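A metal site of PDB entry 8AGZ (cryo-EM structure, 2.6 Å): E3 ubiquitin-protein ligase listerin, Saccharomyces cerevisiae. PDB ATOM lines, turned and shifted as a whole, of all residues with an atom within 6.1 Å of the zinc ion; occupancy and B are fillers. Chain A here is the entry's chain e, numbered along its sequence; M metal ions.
Within 4 Å of the zinc ion: Cys 1508, Cys 1511, His 1535 and Cys 1538. The nearest printed residue that does not touch the zinc ion is Ile 1510 (4.2 Å).
The zinc ion is bound by ND1 of His 1535, SG of Cys 1508, SG of Cys 1538 and SG of Cys 1511.
The side-chain sulfur of Cys 1511 sits close to the side-chain hydroxyl of Ser 1513 (3.2 Å). The side-chain sulfur of Cys 1508 sits close to the backbone NH of Ile 1510 (3.4 Å). The backbone carbonyl oxygen (O) of Ser 1513 is in hydrogen-bond range of a ring nitrogen (NE2) of His 1535. A ring nitrogen (NE2) of His 1535 lies within hydrogen-bond range of the backbone NH (N) of His 1516, at 3.1 Å. O of Ser 1513 sits at hydrogen-bond distance from N of Cys 1508 (3.0 Å).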
ATOM      1  N   CYS A1508     -16.941  15.397  26.738  1.00  0.00           N
ATOM      2  CA  CYS A1508     -17.925  14.412  26.345  1.00  0.00           C
ATOM      3  C   CYS A1508     -18.261  13.634  27.592  1.00  0.00           C
ATOM      4  O   CYS A1508     -17.370  13.246  28.332  1.00  0.00           O
ATOM      5  CB  CYS A1508     -17.354  13.489  25.308  1.00  0.00           C
ATOM      6  SG  CYS A1508     -18.082  11.842  25.210  1.00  0.00           S
ATOM      7  N   ALA A1509     -19.536  13.395  27.819  1.00  0.00           N
ATOM      8  CA  ALA A1509     -19.945  12.720  29.044  1.00  0.00           C
ATOM      9  C   ALA A1509     -19.414  11.308  29.138  1.00  0.00           C
ATOM     10  O   ALA A1509     -18.982  10.875  30.206  1.00  0.00           O
ATOM     11  CB  ALA A1509     -21.455  12.720  29.145  1.00  0.00           C
ATOM     12  N   ILE A1510     -19.434  10.595  28.025  1.00  0.00           N
ATOM     13  CA  ILE A1510     -19.037   9.193  28.074  1.00  0.00           C
ATOM     14  C   ILE A1510     -17.593   8.991  28.512  1.00  0.00           C
ATOM     15  O   ILE A1510     -17.311   8.123  29.350  1.00  0.00           O
ATOM     16  CB  ILE A1510     -19.261   8.512  26.714  1.00  0.00           C
ATOM     17  CG1 ILE A1510     -20.691   8.778  26.222  1.00  0.00           C
ATOM     18  CG2 ILE A1510     -18.994   7.015  26.797  1.00  0.00           C
ATOM     19  CD1 ILE A1510     -21.044   8.030  24.953  1.00  0.00           C
ATOM     20  N   CYS A1511     -16.669   9.768  27.977  1.00  0.00           N
ATOM     21  CA  CYS A1511     -15.269   9.555  28.296  1.00  0.00           C
ATOM     22  C   CYS A1511     -14.657  10.645  29.158  1.00  0.00           C
ATOM     23  O   CYS A1511     -13.471  10.567  29.488  1.00  0.00           O
ATOM     24  CB  CYS A1511     -14.476   9.412  27.009  1.00  0.00           C
ATOM     25  SG  CYS A1511     -14.682  10.825  25.908  1.00  0.00           S
ATOM     26  N   TYR A1512     -15.436  11.662  29.493  1.00  0.00           N
ATOM     27  CA  TYR A1512     -14.955  12.785  30.304  1.00  0.00           C
ATOM     28  C   TYR A1512     -13.712  13.471  29.736  1.00  0.00           C
ATOM     29  O   TYR A1512     -12.819  13.868  30.483  1.00  0.00           O
ATOM     30  CB  TYR A1512     -14.756  12.379  31.763  1.00  0.00           C
ATOM     31  CG  TYR A1512     -15.143  13.485  32.717  1.00  0.00           C
ATOM     32  CD1 TYR A1512     -16.315  14.198  32.545  1.00  0.00           C
ATOM     33  CD2 TYR A1512     -14.323  13.816  33.797  1.00  0.00           C
ATOM     34  CE1 TYR A1512     -16.672  15.207  33.402  1.00  0.00           C
ATOM     35  CE2 TYR A1512     -14.682  14.824  34.667  1.00  0.00           C
ATOM     36  CZ  TYR A1512     -15.850  15.520  34.467  1.00  0.00           C
ATOM     37  OH  TYR A1512     -16.212  16.524  35.330  1.00  0.00           O
ATOM     38  N   SER A1513     -13.639  13.603  28.414  1.00  0.00           N
ATOM     39  CA  SER A1513     -12.538  14.321  27.786  1.00  0.00           C
ATOM     40  C   SER A1513     -13.174  15.247  26.770  1.00  0.00           C
ATOM     41  O   SER A1513     -14.089  14.860  26.063  1.00  0.00           O
ATOM     42  CB  SER A1513     -11.576  13.368  27.089  1.00  0.00           C
ATOM     43  OG  SER A1513     -12.179  12.777  25.948  1.00  0.00           O
ATOM     44  N   HIS A1516     -12.240  14.306  21.325  1.00  0.00           N
ATOM     45  CA  HIS A1516     -12.452  12.908  20.972  1.00  0.00           C
ATOM     46  C   HIS A1516     -11.086  12.315  20.920  1.00  0.00           C
ATOM     47  O   HIS A1516     -10.164  12.931  20.390  1.00  0.00           O
ATOM     48  CB  HIS A1516     -13.166  12.778  19.630  1.00  0.00           C
ATOM     49  CG  HIS A1516     -13.524  11.376  19.259  1.00  0.00           C
ATOM     50  ND1 HIS A1516     -12.931  10.714  18.213  1.00  0.00           N
ATOM     51  CD2 HIS A1516     -14.396  10.501  19.820  1.00  0.00           C
ATOM     52  CE1 HIS A1516     -13.434   9.487  18.126  1.00  0.00           C
ATOM     53  NE2 HIS A1516     -14.319   9.336  19.092  1.00  0.00           N
ATOM     54  N   PHE A1534     -21.602  15.249  24.243  1.00  0.00           N
ATOM     55  CA  PHE A1534     -21.127  13.921  23.846  1.00  0.00           C
ATOM     56  C   PHE A1534     -20.322  13.992  22.564  1.00  0.00           C
ATOM     57  O   PHE A1534     -20.686  14.726  21.636  1.00  0.00           O
ATOM     58  CB  PHE A1534     -22.309  12.977  23.621  1.00  0.00           C
ATOM     59  CG  PHE A1534     -23.157  12.745  24.833  1.00  0.00           C
ATOM     60  CD1 PHE A1534     -24.235  13.583  25.123  1.00  0.00           C
ATOM     61  CD2 PHE A1534     -22.913  11.680  25.679  1.00  0.00           C
ATOM     62  CE1 PHE A1534     -25.018  13.375  26.236  1.00  0.00           C
ATOM     63  CE2 PHE A1534     -23.703  11.461  26.791  1.00  0.00           C
ATOM     64  CZ  PHE A1534     -24.753  12.305  27.077  1.00  0.00           C
ATOM     65  N   HIS A1535     -19.234  13.233  22.461  1.00  0.00           N
ATOM     66  CA  HIS A1535     -18.464  13.188  21.216  1.00  0.00           C
ATOM     67  C   HIS A1535     -19.346  12.608  20.140  1.00  0.00           C
ATOM     68  O   HIS A1535     -20.128  11.708  20.406  1.00  0.00           O
ATOM     69  CB  HIS A1535     -17.243  12.308  21.349  1.00  0.00           C
ATOM     70  CG  HIS A1535     -16.145  12.911  22.173  1.00  0.00           C
ATOM     71  ND1 HIS A1535     -15.453  12.201  23.134  1.00  0.00           N
ATOM     72  CD2 HIS A1535     -15.664  14.167  22.195  1.00  0.00           C
ATOM     73  CE1 HIS A1535     -14.554  12.999  23.680  1.00  0.00           C
ATOM     74  NE2 HIS A1535     -14.683  14.196  23.148  1.00  0.00           N
ATOM     75  N   CYS A1538     -18.627   8.975  19.658  1.00  0.00           N
ATOM     76  CA  CYS A1538     -18.980   8.278  20.891  1.00  0.00           C
ATOM     77  C   CYS A1538     -20.487   8.140  20.990  1.00  0.00           C
ATOM     78  O   CYS A1538     -20.991   7.077  21.359  1.00  0.00           O
ATOM     79  CB  CYS A1538     -18.523   9.080  22.116  1.00  0.00           C
ATOM     80  SG  CYS A1538     -16.778   8.952  22.598  1.00  0.00           S
HETATM   81 ZN    ZN M   1     -16.396  10.477  24.334  1.00  0.00          ZN
